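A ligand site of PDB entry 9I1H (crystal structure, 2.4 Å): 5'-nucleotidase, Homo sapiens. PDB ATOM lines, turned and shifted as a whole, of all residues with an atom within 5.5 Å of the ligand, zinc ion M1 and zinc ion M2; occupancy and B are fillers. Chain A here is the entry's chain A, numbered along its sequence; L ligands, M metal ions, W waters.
O5 of the ligand is bound to zinc ion M2 (1.9 Å). Zinc ion M2 is bound by a ring nitrogen (NE2) of His 220 (2.3 Å). ND1 of His 243 binds zinc ion M2, at 2.3 Å. OD2 of Asp 85 is bound to zinc ion M2 (2.4 Å). ND2 of Asn 117 is bound to zinc ion M2 (2.4 Å). Zinc ion M2 has five donor atoms within binding distance.
Three residues have an atom within 4 Å of zinc ion M1: Asp 36, His 38 and Asp 85. The nearest printed residue that does not touch zinc ion M1 is Asn 245 (4.1 Å).
The backbone carbonyl oxygen (O) of Gly 392 lies close to an oxygen (O3) of the ligand, 3.3 Å away. OD1 of Asp 121 touches C15 of the ligand, 3.9 Å away. Leu 184 touches the ligand (O to C17, 3.4 Å). Ser 185 touches the ligand. Asn 186 touches the ligand. CA of Gly 393 touches N1 of the ligand, at 3.8 Å. Phe 417 touches the ligand (CD2 to C5, 3.2 Å). Gly 419 touches the ligand (CA to C13, 3.9 Å). CA of Gly 447 touches O1 of the ligand (3.3 Å). ND2 of Asn 499 touches C13 of the ligand (3.3 Å). Phe 500 touches the ligand. Hydrophobic or aromatic side chains within 4 Å of the ligand: His 38, His 118, His 243, Phe 417 and Phe 500. 22 residues have an atom within 4 Å of the ligand: Asp 36, His 38, Asp 85, Asn 117, His 118, Asp 121, Leu 184, Ser 185, Asn 186, His 243, Asn 245, Arg 354, Asn 390, Gly 392, Gly 393, Arg 395, Phe 417, Gly 419, Gly 447, Asn 499, Phe 500 and Asp 506. The nearest printed residue that does not touch the ligand is Pro 498 (4.1 Å).
The side-chain carboxylate of Asp 36 lies within hydrogen-bond range of the backbone NH of His 243 (2.8 Å). N of His 118 lies within hydrogen-bond range of OD1 of Asp 85. A ring nitrogen (NE2) of His 38 lies close to the guanidinium group (NH2) of Arg 395, 3.4 Å away. OD2 of Asp 121 is in hydrogen-bond range of ND1 of His 118 (2.8 Å). NH1 of Arg 354 is in hydrogen-bond range of O of Ser 445 (3.3 Å). The side-chain amide nitrogen (ND2) of Asn 390 lies close to the backbone NH (N) of Gly 393 (3.2 Å). O of Gly 447 sits at hydrogen-bond distance from N of Gly 392, at 2.9 Å. The backbone NH of Asp 121 sits at hydrogen-bond distance from the side-chain hydroxyl of Ser 185, 3.2 Å away.
The side-chain carboxylate (OD2) of Asp 506 sits at hydrogen-bond distance from an oxygen (O2) of the ligand (2.4 Å). NE2 of His 118 is in hydrogen-bond range of O7 of the ligand, at 2.6 Å. An oxygen (O9) of the ligand is in hydrogen-bond range of the side-chain amide nitrogen (ND2) of Asn 245, at 2.9 Å. NH1 of Arg 395 lies within salt-bridge range of O7 of the ligand, 3.1 Å away. NH1 of Arg 354 lies within salt-bridge range of O8 of the ligand, 3.1 Å away. An oxygen (O2) of the ligand sits at hydrogen-bond distance from the side-chain amide nitrogen (ND2) of Asn 390.
Five residues have an atom within 4 Å of zinc ion M2: Asp 36, Asp 85, Asn 117, His 220 and His 243. The nearest printed residue that does not touch zinc ion M2 is His 118 (4.05 Å).
Water W1 lies within hydrogen-bond range of N4 of the ligand (2.7 Å) and OD1 of Asn 499 (3.4 Å).
The side-chain carboxylate (OD1) of Asp 36 is bound to zinc ion M1 (2.0 Å). Zinc ion M1 is bound by O6 of the ligand, at 2.1 Å. Zinc ion M1 is bound by OD2 of Asp 85, at 2.2 Å. Zinc ion M1 is bound by NE2 of His 38 (2.3 Å).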
ATOM      1  N   ASP A  36      -5.487  20.367 -16.288  1.00  0.00           N
ATOM      2  CA  ASP A  36      -4.961  19.271 -15.475  1.00  0.00           C
ATOM      3  C   ASP A  36      -3.644  19.675 -14.812  1.00  0.00           C
ATOM      4  O   ASP A  36      -2.665  18.931 -14.807  1.00  0.00           O
ATOM      5  CB  ASP A  36      -4.795  18.004 -16.310  1.00  0.00           C
ATOM      6  CG  ASP A  36      -6.135  17.431 -16.775  1.00  0.00           C
ATOM      7  OD1 ASP A  36      -6.906  16.926 -15.934  1.00  0.00           O
ATOM      8  OD2 ASP A  36      -6.433  17.517 -17.984  1.00  0.00           O
ATOM      9  N   HIS A  38      -3.138  20.130 -11.629  1.00  0.00           N
ATOM     10  CA  HIS A  38      -3.000  19.170 -10.535  1.00  0.00           C
ATOM     11  C   HIS A  38      -1.986  19.637  -9.482  1.00  0.00           C
ATOM     12  O   HIS A  38      -1.066  18.903  -9.110  1.00  0.00           O
ATOM     13  CB  HIS A  38      -2.636  17.789 -11.073  1.00  0.00           C
ATOM     14  CG  HIS A  38      -3.808  17.025 -11.604  1.00  0.00           C
ATOM     15  ND1 HIS A  38      -4.944  16.794 -10.844  1.00  0.00           N
ATOM     16  CD2 HIS A  38      -4.040  16.444 -12.801  1.00  0.00           C
ATOM     17  CE1 HIS A  38      -5.816  16.104 -11.559  1.00  0.00           C
ATOM     18  NE2 HIS A  38      -5.282  15.876 -12.748  1.00  0.00           N
ATOM     19  N   ASP A  85      -9.385  20.554 -13.284  1.00  0.00           N
ATOM     20  CA  ASP A  85      -8.428  19.669 -12.611  1.00  0.00           C
ATOM     21  C   ASP A  85      -7.214  20.438 -12.080  1.00  0.00           C
ATOM     22  O   ASP A  85      -6.064  20.071 -12.322  1.00  0.00           O
ATOM     23  CB  ASP A  85      -7.984  18.523 -13.525  1.00  0.00           C
ATOM     24  CG  ASP A  85      -8.891  17.319 -13.437  1.00  0.00           C
ATOM     25  OD1 ASP A  85      -9.961  17.412 -12.788  1.00  0.00           O
ATOM     26  OD2 ASP A  85      -8.538  16.260 -13.991  1.00  0.00           O
ATOM     27  N   ASN A 117     -13.623  16.930 -12.808  1.00  0.00           N
ATOM     28  CA  ASN A 117     -14.151  15.942 -11.862  1.00  0.00           C
ATOM     29  C   ASN A 117     -13.433  16.023 -10.523  1.00  0.00           C
ATOM     30  O   ASN A 117     -14.082  16.029  -9.465  1.00  0.00           O
ATOM     31  CB  ASN A 117     -14.044  14.535 -12.450  1.00  0.00           C
ATOM     32  CG  ASN A 117     -12.633  14.168 -12.855  1.00  0.00           C
ATOM     33  OD1 ASN A 117     -11.854  13.650 -12.041  1.00  0.00           O
ATOM     34  ND2 ASN A 117     -12.284  14.415 -14.110  1.00  0.00           N
ATOM     35  N   HIS A 118     -12.101  16.115 -10.535  1.00  0.00           N
ATOM     36  CA  HIS A 118     -11.358  16.159  -9.284  1.00  0.00           C
ATOM     37  C   HIS A 118     -11.667  17.393  -8.451  1.00  0.00           C
ATOM     38  O   HIS A 118     -11.328  17.419  -7.258  1.00  0.00           O
ATOM     39  CB  HIS A 118      -9.847  16.079  -9.553  1.00  0.00           C
ATOM     40  CG  HIS A 118      -9.366  14.710  -9.918  1.00  0.00           C
ATOM     41  ND1 HIS A 118      -9.215  13.699  -8.993  1.00  0.00           N
ATOM     42  CD2 HIS A 118      -8.983  14.185 -11.104  1.00  0.00           C
ATOM     43  CE1 HIS A 118      -8.763  12.611  -9.598  1.00  0.00           C
ATOM     44  NE2 HIS A 118      -8.623  12.881 -10.879  1.00  0.00           N
ATOM     45  N   ASP A 121     -13.485  16.214  -5.530  1.00  0.00           N
ATOM     46  CA  ASP A 121     -12.858  15.157  -4.744  1.00  0.00           C
ATOM     47  C   ASP A 121     -13.200  15.289  -3.266  1.00  0.00           C
ATOM     48  O   ASP A 121     -13.349  14.275  -2.574  1.00  0.00           O
ATOM     49  CB  ASP A 121     -11.339  15.196  -4.925  1.00  0.00           C
ATOM     50  CG  ASP A 121     -10.871  14.354  -6.100  1.00  0.00           C
ATOM     51  OD1 ASP A 121     -11.718  13.820  -6.850  1.00  0.00           O
ATOM     52  OD2 ASP A 121      -9.640  14.216  -6.276  1.00  0.00           O
ATOM     53  N   PHE A 183     -19.305   8.917 -11.013  1.00  0.00           N
ATOM     54  CA  PHE A 183     -18.527   7.698 -10.832  1.00  0.00           C
ATOM     55  C   PHE A 183     -17.055   7.982 -10.558  1.00  0.00           C
ATOM     56  O   PHE A 183     -16.391   7.138  -9.960  1.00  0.00           O
ATOM     57  CB  PHE A 183     -18.665   6.812 -12.081  1.00  0.00           C
ATOM     58  CG  PHE A 183     -20.091   6.531 -12.478  1.00  0.00           C
ATOM     59  CD1 PHE A 183     -20.804   7.451 -13.238  1.00  0.00           C
ATOM     60  CD2 PHE A 183     -20.717   5.361 -12.090  1.00  0.00           C
ATOM     61  CE1 PHE A 183     -22.110   7.204 -13.607  1.00  0.00           C
ATOM     62  CE2 PHE A 183     -22.023   5.114 -12.459  1.00  0.00           C
ATOM     63  CZ  PHE A 183     -22.727   6.036 -13.222  1.00  0.00           C
ATOM     64  N   LEU A 184     -16.557   9.144 -10.985  1.00  0.00           N
ATOM     65  CA  LEU A 184     -15.132   9.462 -10.865  1.00  0.00           C
ATOM     66  C   LEU A 184     -14.779  10.211  -9.592  1.00  0.00           C
ATOM     67  O   LEU A 184     -13.584  10.371  -9.306  1.00  0.00           O
ATOM     68  CB  LEU A 184     -14.679  10.311 -12.056  1.00  0.00           C
ATOM     69  CG  LEU A 184     -14.841   9.770 -13.476  1.00  0.00           C
ATOM     70  CD1 LEU A 184     -14.279  10.758 -14.485  1.00  0.00           C
ATOM     71  CD2 LEU A 184     -14.152   8.424 -13.611  1.00  0.00           C
ATOM     72  N   SER A 185     -15.755  10.687  -8.818  1.00  0.00           N
ATOM     73  CA  SER A 185     -15.427  11.618  -7.751  1.00  0.00           C
ATOM     74  C   SER A 185     -16.558  11.594  -6.708  1.00  0.00           C
ATOM     75  O   SER A 185     -17.227  10.571  -6.539  1.00  0.00           O
ATOM     76  CB  SER A 185     -15.161  13.014  -8.345  1.00  0.00           C
ATOM     77  OG  SER A 185     -15.026  13.998  -7.333  1.00  0.00           O
ATOM     78  N   ASN A 186     -16.769  12.741  -6.043  1.00  0.00           N
ATOM     79  CA  ASN A 186     -17.664  12.816  -4.891  1.00  0.00           C
ATOM     80  C   ASN A 186     -18.607  14.014  -4.996  1.00  0.00           C
ATOM     81  O   ASN A 186     -18.729  14.813  -4.059  1.00  0.00           O
ATOM     82  CB  ASN A 186     -16.839  12.884  -3.600  1.00  0.00           C
ATOM     83  CG  ASN A 186     -16.842  11.585  -2.845  1.00  0.00           C
ATOM     84  OD1 ASN A 186     -17.897  10.997  -2.594  1.00  0.00           O
ATOM     85  ND2 ASN A 186     -15.662  11.130  -2.454  1.00  0.00           N
ATOM     86  N   HIS A 220     -14.324  19.757 -19.620  1.00  0.00           N
ATOM     87  CA  HIS A 220     -13.492  18.730 -19.013  1.00  0.00           C
ATOM     88  C   HIS A 220     -14.188  17.374 -19.164  1.00  0.00           C
ATOM     89  O   HIS A 220     -14.878  16.891 -18.258  1.00  0.00           O
ATOM     90  CB  HIS A 220     -13.205  19.051 -17.546  1.00  0.00           C
ATOM     91  CG  HIS A 220     -12.188  18.170 -16.920  1.00  0.00           C
ATOM     92  ND1 HIS A 220     -10.839  18.466 -16.954  1.00  0.00           N
ATOM     93  CD2 HIS A 220     -12.309  16.988 -16.276  1.00  0.00           C
ATOM     94  CE1 HIS A 220     -10.181  17.504 -16.332  1.00  0.00           C
ATOM     95  NE2 HIS A 220     -11.049  16.595 -15.920  1.00  0.00           N
ATOM     96  N   HIS A 243      -8.753  16.642 -19.295  1.00  0.00           N
ATOM     97  CA  HIS A 243      -9.175  15.379 -18.678  1.00  0.00           C
ATOM     98  C   HIS A 243      -8.454  14.154 -19.225  1.00  0.00           C
ATOM     99  O   HIS A 243      -8.377  13.129 -18.549  1.00  0.00           O
ATOM    100  CB  HIS A 243     -10.681  15.165 -18.832  1.00  0.00           C
ATOM    101  CG  HIS A 243     -11.173  13.927 -18.145  1.00  0.00           C
ATOM    102  ND1 HIS A 243     -11.070  13.737 -16.781  1.00  0.00           N
ATOM    103  CD2 HIS A 243     -11.778  12.814 -18.632  1.00  0.00           C
ATOM    104  CE1 HIS A 243     -11.588  12.570 -16.461  1.00  0.00           C
ATOM    105  NE2 HIS A 243     -12.029  11.993 -17.562  1.00  0.00           N
ATOM    106  N   SER A 244      -7.933  14.226 -20.453  1.00  0.00           N
ATOM    107  CA  SER A 244      -7.210  13.111 -21.042  1.00  0.00           C
ATOM    108  C   SER A 244      -5.720  13.405 -21.215  1.00  0.00           C
ATOM    109  O   SER A 244      -5.017  12.606 -21.850  1.00  0.00           O
ATOM    110  CB  SER A 244      -7.844  12.741 -22.384  1.00  0.00           C
ATOM    111  OG  SER A 244      -8.005  13.883 -23.200  1.00  0.00           O
ATOM    112  N   ASN A 245      -5.241  14.510 -20.655  1.00  0.00           N
ATOM    113  CA  ASN A 245      -3.835  14.898 -20.743  1.00  0.00           C
ATOM    114  C   ASN A 245      -3.306  14.763 -22.178  1.00  0.00           C
ATOM    115  O   ASN A 245      -2.224  14.230 -22.428  1.00  0.00           O
ATOM    116  CB  ASN A 245      -3.011  14.076 -19.759  1.00  0.00           C
ATOM    117  CG  ASN A 245      -3.594  14.085 -18.356  1.00  0.00           C
ATOM    118  OD1 ASN A 245      -4.161  15.087 -17.912  1.00  0.00           O
ATOM    119  ND2 ASN A 245      -3.497  12.961 -17.659  1.00  0.00           N
ATOM    120  N   ARG A 354       0.778   2.674 -17.475  1.00  0.00           N
ATOM    121  CA  ARG A 354      -0.458   2.406 -18.218  1.00  0.00           C
ATOM    122  C   ARG A 354      -0.197   1.617 -19.491  1.00  0.00           C
ATOM    123  O   ARG A 354      -1.123   1.424 -20.286  1.00  0.00           O
ATOM    124  CB  ARG A 354      -1.177   3.712 -18.553  1.00  0.00           C
ATOM    125  CG  ARG A 354      -1.585   4.504 -17.332  1.00  0.00           C
ATOM    126  CD  ARG A 354      -2.472   5.681 -17.686  1.00  0.00           C
ATOM    127  NE  ARG A 354      -2.584   6.595 -16.558  1.00  0.00           N
ATOM    128  CZ  ARG A 354      -3.524   7.509 -16.405  1.00  0.00           C
ATOM    129  NH1 ARG A 354      -4.503   7.657 -17.296  1.00  0.00           N
ATOM    130  NH2 ARG A 354      -3.496   8.303 -15.338  1.00  0.00           N
ATOM    131  N   ASN A 390      -4.501  -0.473 -10.271  1.00  0.00           N
ATOM    132  CA  ASN A 390      -4.765   0.258 -11.502  1.00  0.00           C
ATOM    133  C   ASN A 390      -3.659   1.273 -11.763  1.00  0.00           C
ATOM    134  O   ASN A 390      -3.402   2.153 -10.928  1.00  0.00           O
ATOM    135  CB  ASN A 390      -6.133   0.930 -11.430  1.00  0.00           C
ATOM    136  CG  ASN A 390      -6.293   1.791 -10.189  1.00  0.00           C
ATOM    137  OD1 ASN A 390      -6.334   1.280  -9.060  1.00  0.00           O
ATOM    138  ND2 ASN A 390      -6.405   3.102 -10.376  1.00  0.00           N
ATOM    139  N   GLY A 391      -3.006   1.157 -12.927  1.00  0.00           N
ATOM    140  CA  GLY A 391      -1.866   2.003 -13.216  1.00  0.00           C
ATOM    141  C   GLY A 391      -2.178   3.479 -13.116  1.00  0.00           C
ATOM    142  O   GLY A 391      -1.357   4.277 -12.679  1.00  0.00           O
ATOM    143  N   GLY A 392      -3.381   3.871 -13.529  1.00  0.00           N
ATOM    144  CA  GLY A 392      -3.774   5.262 -13.451  1.00  0.00           C
ATOM    145  C   GLY A 392      -3.782   5.812 -12.046  1.00  0.00           C
ATOM    146  O   GLY A 392      -3.769   7.042 -11.870  1.00  0.00           O
ATOM    147  N   GLY A 393      -3.810   4.940 -11.029  1.00  0.00           N
ATOM    148  CA  GLY A 393      -3.744   5.381  -9.655  1.00  0.00           C
ATOM    149  C   GLY A 393      -2.361   5.789  -9.186  1.00  0.00           C
ATOM    150  O   GLY A 393      -2.236   6.383  -8.111  1.00  0.00           O
ATOM    151  N   ARG A 395       0.184   8.376  -9.636  1.00  0.00           N
ATOM    152  CA  ARG A 395      -0.013   9.724 -10.161  1.00  0.00           C
ATOM    153  C   ARG A 395       1.282  10.528 -10.303  1.00  0.00           C
ATOM    154  O   ARG A 395       1.212  11.684 -10.717  1.00  0.00           O
ATOM    155  CB  ARG A 395      -0.995  10.497  -9.268  1.00  0.00           C
ATOM    156  CG  ARG A 395      -2.346   9.824  -9.032  1.00  0.00           C
ATOM    157  CD  ARG A 395      -3.279   9.845 -10.254  1.00  0.00           C
ATOM    158  NE  ARG A 395      -3.740  11.192 -10.592  1.00  0.00           N
ATOM    159  CZ  ARG A 395      -4.745  11.452 -11.407  1.00  0.00           C
ATOM    160  NH1 ARG A 395      -5.430  10.486 -11.994  1.00  0.00           N
ATOM    161  NH2 ARG A 395      -5.077  12.717 -11.642  1.00  0.00           N
ATOM    162  N   PHE A 417      -4.817  10.626  -3.350  1.00  0.00           N
ATOM    163  CA  PHE A 417      -6.257  10.563  -3.105  1.00  0.00           C
ATOM    164  C   PHE A 417      -6.625  10.119  -1.696  1.00  0.00           C
ATOM    165  O   PHE A 417      -7.731  10.404  -1.244  1.00  0.00           O
ATOM    166  CB  PHE A 417      -6.922   9.628  -4.115  1.00  0.00           C
ATOM    167  CG  PHE A 417      -6.686  10.012  -5.548  1.00  0.00           C
ATOM    168  CD1 PHE A 417      -6.892  11.304  -5.977  1.00  0.00           C
ATOM    169  CD2 PHE A 417      -6.262   9.060  -6.471  1.00  0.00           C
ATOM    170  CE1 PHE A 417      -6.678  11.655  -7.300  1.00  0.00           C
ATOM    171  CE2 PHE A 417      -6.057   9.408  -7.791  1.00  0.00           C
ATOM    172  CZ  PHE A 417      -6.271  10.702  -8.209  1.00  0.00           C
ATOM    173  N   GLY A 418      -5.739   9.410  -1.003  1.00  0.00           N
ATOM    174  CA  GLY A 418      -6.064   8.951   0.326  1.00  0.00           C
ATOM    175  C   GLY A 418      -7.022   7.784   0.383  1.00  0.00           C
ATOM    176  O   GLY A 418      -7.785   7.666   1.354  1.00  0.00           O
ATOM    177  N   GLY A 419      -7.033   6.935  -0.638  1.00  0.00           N
ATOM    178  CA  GLY A 419      -7.775   5.697  -0.567  1.00  0.00           C
ATOM    179  C   GLY A 419      -7.094   4.716   0.386  1.00  0.00           C
ATOM    180  O   GLY A 419      -6.116   5.032   1.067  1.00  0.00           O
ATOM    181  N   SER A 445      -3.552   4.989 -23.276  1.00  0.00           N
ATOM    182  CA  SER A 445      -3.070   5.553 -22.019  1.00  0.00           C
ATOM    183  C   SER A 445      -4.225   5.725 -21.031  1.00  0.00           C
ATOM    184  O   SER A 445      -4.416   6.795 -20.435  1.00  0.00           O
ATOM    185  CB  SER A 445      -2.340   6.876 -22.264  1.00  0.00           C
ATOM    186  OG  SER A 445      -1.557   7.239 -21.139  1.00  0.00           O
ATOM    187  N   THR A 446      -5.006   4.669 -20.869  1.00  0.00           N
ATOM    188  CA  THR A 446      -6.116   4.644 -19.931  1.00  0.00           C
ATOM    189  C   THR A 446      -5.671   4.030 -18.612  1.00  0.00           C
ATOM    190  O   THR A 446      -4.787   3.163 -18.563  1.00  0.00           O
ATOM    191  CB  THR A 446      -7.305   3.861 -20.495  1.00  0.00           C
ATOM    192  OG1 THR A 446      -6.883   2.532 -20.844  1.00  0.00           O
ATOM    193  CG2 THR A 446      -7.865   4.571 -21.725  1.00  0.00           C
ATOM    194  N   GLY A 447      -6.321   4.457 -17.529  1.00  0.00           N
ATOM    195  CA  GLY A 447      -5.856   4.117 -16.199  1.00  0.00           C
ATOM    196  C   GLY A 447      -6.077   2.669 -15.780  1.00  0.00           C
ATOM    197  O   GLY A 447      -5.460   2.237 -14.795  1.00  0.00           O
ATOM    198  N   GLU A 448      -6.911   1.914 -16.494  1.00  0.00           N
ATOM    199  CA  GLU A 448      -7.304   0.604 -15.995  1.00  0.00           C
ATOM    200  C   GLU A 448      -6.236  -0.469 -16.210  1.00  0.00           C
ATOM    201  O   GLU A 448      -6.379  -1.565 -15.671  1.00  0.00           O
ATOM    202  CB  GLU A 448      -8.623   0.152 -16.635  1.00  0.00           C
ATOM    203  CG  GLU A 448      -8.586  -0.191 -18.121  1.00  0.00           C
ATOM    204  CD  GLU A 448      -8.827   1.008 -19.005  1.00  0.00           C
ATOM    205  OE1 GLU A 448      -8.905   2.137 -18.482  1.00  0.00           O
ATOM    206  OE2 GLU A 448      -8.951   0.809 -20.236  1.00  0.00           O
ATOM    207  N   PRO A 498      -6.718  -1.637  -4.343  1.00  0.00           N
ATOM    208  CA  PRO A 498      -7.208  -0.351  -3.836  1.00  0.00           C
ATOM    209  C   PRO A 498      -8.709  -0.378  -3.585  1.00  0.00           C
ATOM    210  O   PRO A 498      -9.459  -1.103  -4.251  1.00  0.00           O
ATOM    211  CB  PRO A 498      -6.841   0.633  -4.951  1.00  0.00           C
ATOM    212  CG  PRO A 498      -6.735  -0.209  -6.179  1.00  0.00           C
ATOM    213  CD  PRO A 498      -6.198  -1.534  -5.720  1.00  0.00           C
ATOM    214  N   ASN A 499      -9.150   0.434  -2.626  1.00  0.00           N
ATOM    215  CA  ASN A 499     -10.587   0.638  -2.430  1.00  0.00           C
ATOM    216  C   ASN A 499     -11.253   1.103  -3.714  1.00  0.00           C
ATOM    217  O   ASN A 499     -12.430   0.809  -3.951  1.00  0.00           O
ATOM    218  CB  ASN A 499     -10.824   1.648  -1.313  1.00  0.00           C
ATOM    219  CG  ASN A 499     -10.279   3.038  -1.644  1.00  0.00           C
ATOM    220  OD1 ASN A 499      -9.371   3.191  -2.468  1.00  0.00           O
ATOM    221  ND2 ASN A 499     -10.826   4.054  -0.986  1.00  0.00           N
ATOM    222  N   PHE A 500     -10.506   1.828  -4.555  1.00  0.00           N
ATOM    223  CA  PHE A 500     -11.033   2.335  -5.807  1.00  0.00           C
ATOM    224  C   PHE A 500     -11.524   1.220  -6.720  1.00  0.00           C
ATOM    225  O   PHE A 500     -12.518   1.387  -7.438  1.00  0.00           O
ATOM    226  CB  PHE A 500      -9.950   3.156  -6.500  1.00  0.00           C
ATOM    227  CG  PHE A 500     -10.309   3.624  -7.868  1.00  0.00           C
ATOM    228  CD1 PHE A 500     -11.248   4.636  -8.043  1.00  0.00           C
ATOM    229  CD2 PHE A 500      -9.709   3.064  -8.979  1.00  0.00           C
ATOM    230  CE1 PHE A 500     -11.576   5.066  -9.308  1.00  0.00           C
ATOM    231  CE2 PHE A 500     -10.037   3.494 -10.245  1.00  0.00           C
ATOM    232  CZ  PHE A 500     -10.973   4.497 -10.416  1.00  0.00           C
ATOM    233  N   ASP A 506     -12.787   2.484 -12.476  1.00  0.00           N
ATOM    234  CA  ASP A 506     -12.076   2.271 -13.739  1.00  0.00           C
ATOM    235  C   ASP A 506     -12.770   1.260 -14.629  1.00  0.00           C
ATOM    236  O   ASP A 506     -12.133   0.626 -15.475  1.00  0.00           O
ATOM    237  CB  ASP A 506     -10.623   1.843 -13.483  1.00  0.00           C
ATOM    238  CG  ASP A 506      -9.626   2.981 -13.647  1.00  0.00           C
ATOM    239  OD1 ASP A 506     -10.030   4.108 -14.015  1.00  0.00           O
ATOM    240  OD2 ASP A 506      -8.430   2.749 -13.399  1.00  0.00           O
HETATM  241  N1  LIG L   1      -7.417   5.804  -8.979  1.00  0.00           N
HETATM  242  N2  LIG L   1      -9.641   8.253  -6.403  1.00  0.00           N
HETATM  243  C1  LIG L   1      -7.529   8.910 -14.803  1.00  0.00           C
HETATM  244  C2  LIG L   1      -7.738  11.785 -15.671  1.00  0.00           C
HETATM  245  C3  LIG L   1      -7.963   6.941  -9.414  1.00  0.00           C
HETATM  246  C4  LIG L   1      -7.687   5.619  -7.702  1.00  0.00           C
HETATM  247  C5  LIG L   1      -8.908   7.504  -7.315  1.00  0.00           C
HETATM  248  C6  LIG L   1     -10.514   6.772  -4.592  1.00  0.00           C
HETATM  249  C7  LIG L   1     -11.794   9.496  -6.101  1.00  0.00           C
HETATM  250  C8  LIG L   1     -13.243  10.494  -4.459  1.00  0.00           C
HETATM  251  C9  LIG L   1     -14.068   8.756  -5.865  1.00  0.00           C
HETATM  252  C10 LIG L   1      -8.591   8.643 -10.642  1.00  0.00           C
HETATM  253  N3  LIG L   1      -7.895   7.462 -10.688  1.00  0.00           N
HETATM  254  C11 LIG L   1      -8.374   6.682 -13.879  1.00  0.00           C
HETATM  255  O1  LIG L   1      -8.464   5.854 -15.030  1.00  0.00           O
HETATM  256  C12 LIG L   1      -7.963   5.883 -12.645  1.00  0.00           C
HETATM  257  C13 LIG L   1     -10.622   6.647  -3.094  1.00  0.00           C
HETATM  258  C14 LIG L   1     -10.449   9.410  -6.796  1.00  0.00           C
HETATM  259  C15 LIG L   1     -12.004  10.410  -5.078  1.00  0.00           C
HETATM  260  C16 LIG L   1     -14.267   9.659  -4.851  1.00  0.00           C
HETATM  261  C17 LIG L   1     -12.838   8.670  -6.482  1.00  0.00           C
HETATM  262  C18 LIG L   1      -8.704   7.846  -8.677  1.00  0.00           C
HETATM  263  C19 LIG L   1      -7.168   6.915 -11.830  1.00  0.00           C
HETATM  264  C20 LIG L   1      -7.203   7.648 -14.040  1.00  0.00           C
HETATM  265  C21 LIG L   1      -9.603   7.924  -4.983  1.00  0.00           C
HETATM  266  N4  LIG L   1      -8.383   6.359  -6.850  1.00  0.00           N
HETATM  267  N5  LIG L   1      -9.089   8.926  -9.465  1.00  0.00           N
HETATM  268  O2  LIG L   1      -7.138   4.774 -12.975  1.00  0.00           O
HETATM  269  O3  LIG L   1      -6.837   7.975 -12.693  1.00  0.00           O
HETATM  270  O4  LIG L   1      -6.372   9.760 -14.726  1.00  0.00           O
HETATM  271  O5  LIG L   1      -9.644  13.048 -14.302  1.00  0.00           O
HETATM  272  O6  LIG L   1      -7.279  13.670 -13.836  1.00  0.00           O
HETATM  273  O7  LIG L   1      -8.188  11.467 -12.990  1.00  0.00           O
HETATM  274  O8  LIG L   1      -6.033  10.305 -17.134  1.00  0.00           O
HETATM  275  O9  LIG L   1      -4.901  11.723 -15.422  1.00  0.00           O
HETATM  276  P1  LIG L   1      -6.149  10.954 -15.721  1.00  0.00           P
HETATM  277  P2  LIG L   1      -8.235  12.481 -14.094  1.00  0.00           P
HETATM  278 CL1  LIG L   1      -6.965   4.196  -7.008  1.00  0.00          CL
HETATM  279 ZN    ZN M   1      -6.538  15.453 -14.629  1.00  0.00          ZN
HETATM  280 ZN    ZN M   2     -10.093  14.764 -14.954  1.00  0.00          ZN
HETATM  281  O   HOH W   1      -7.754   5.534  -4.408  1.00  0.00           O
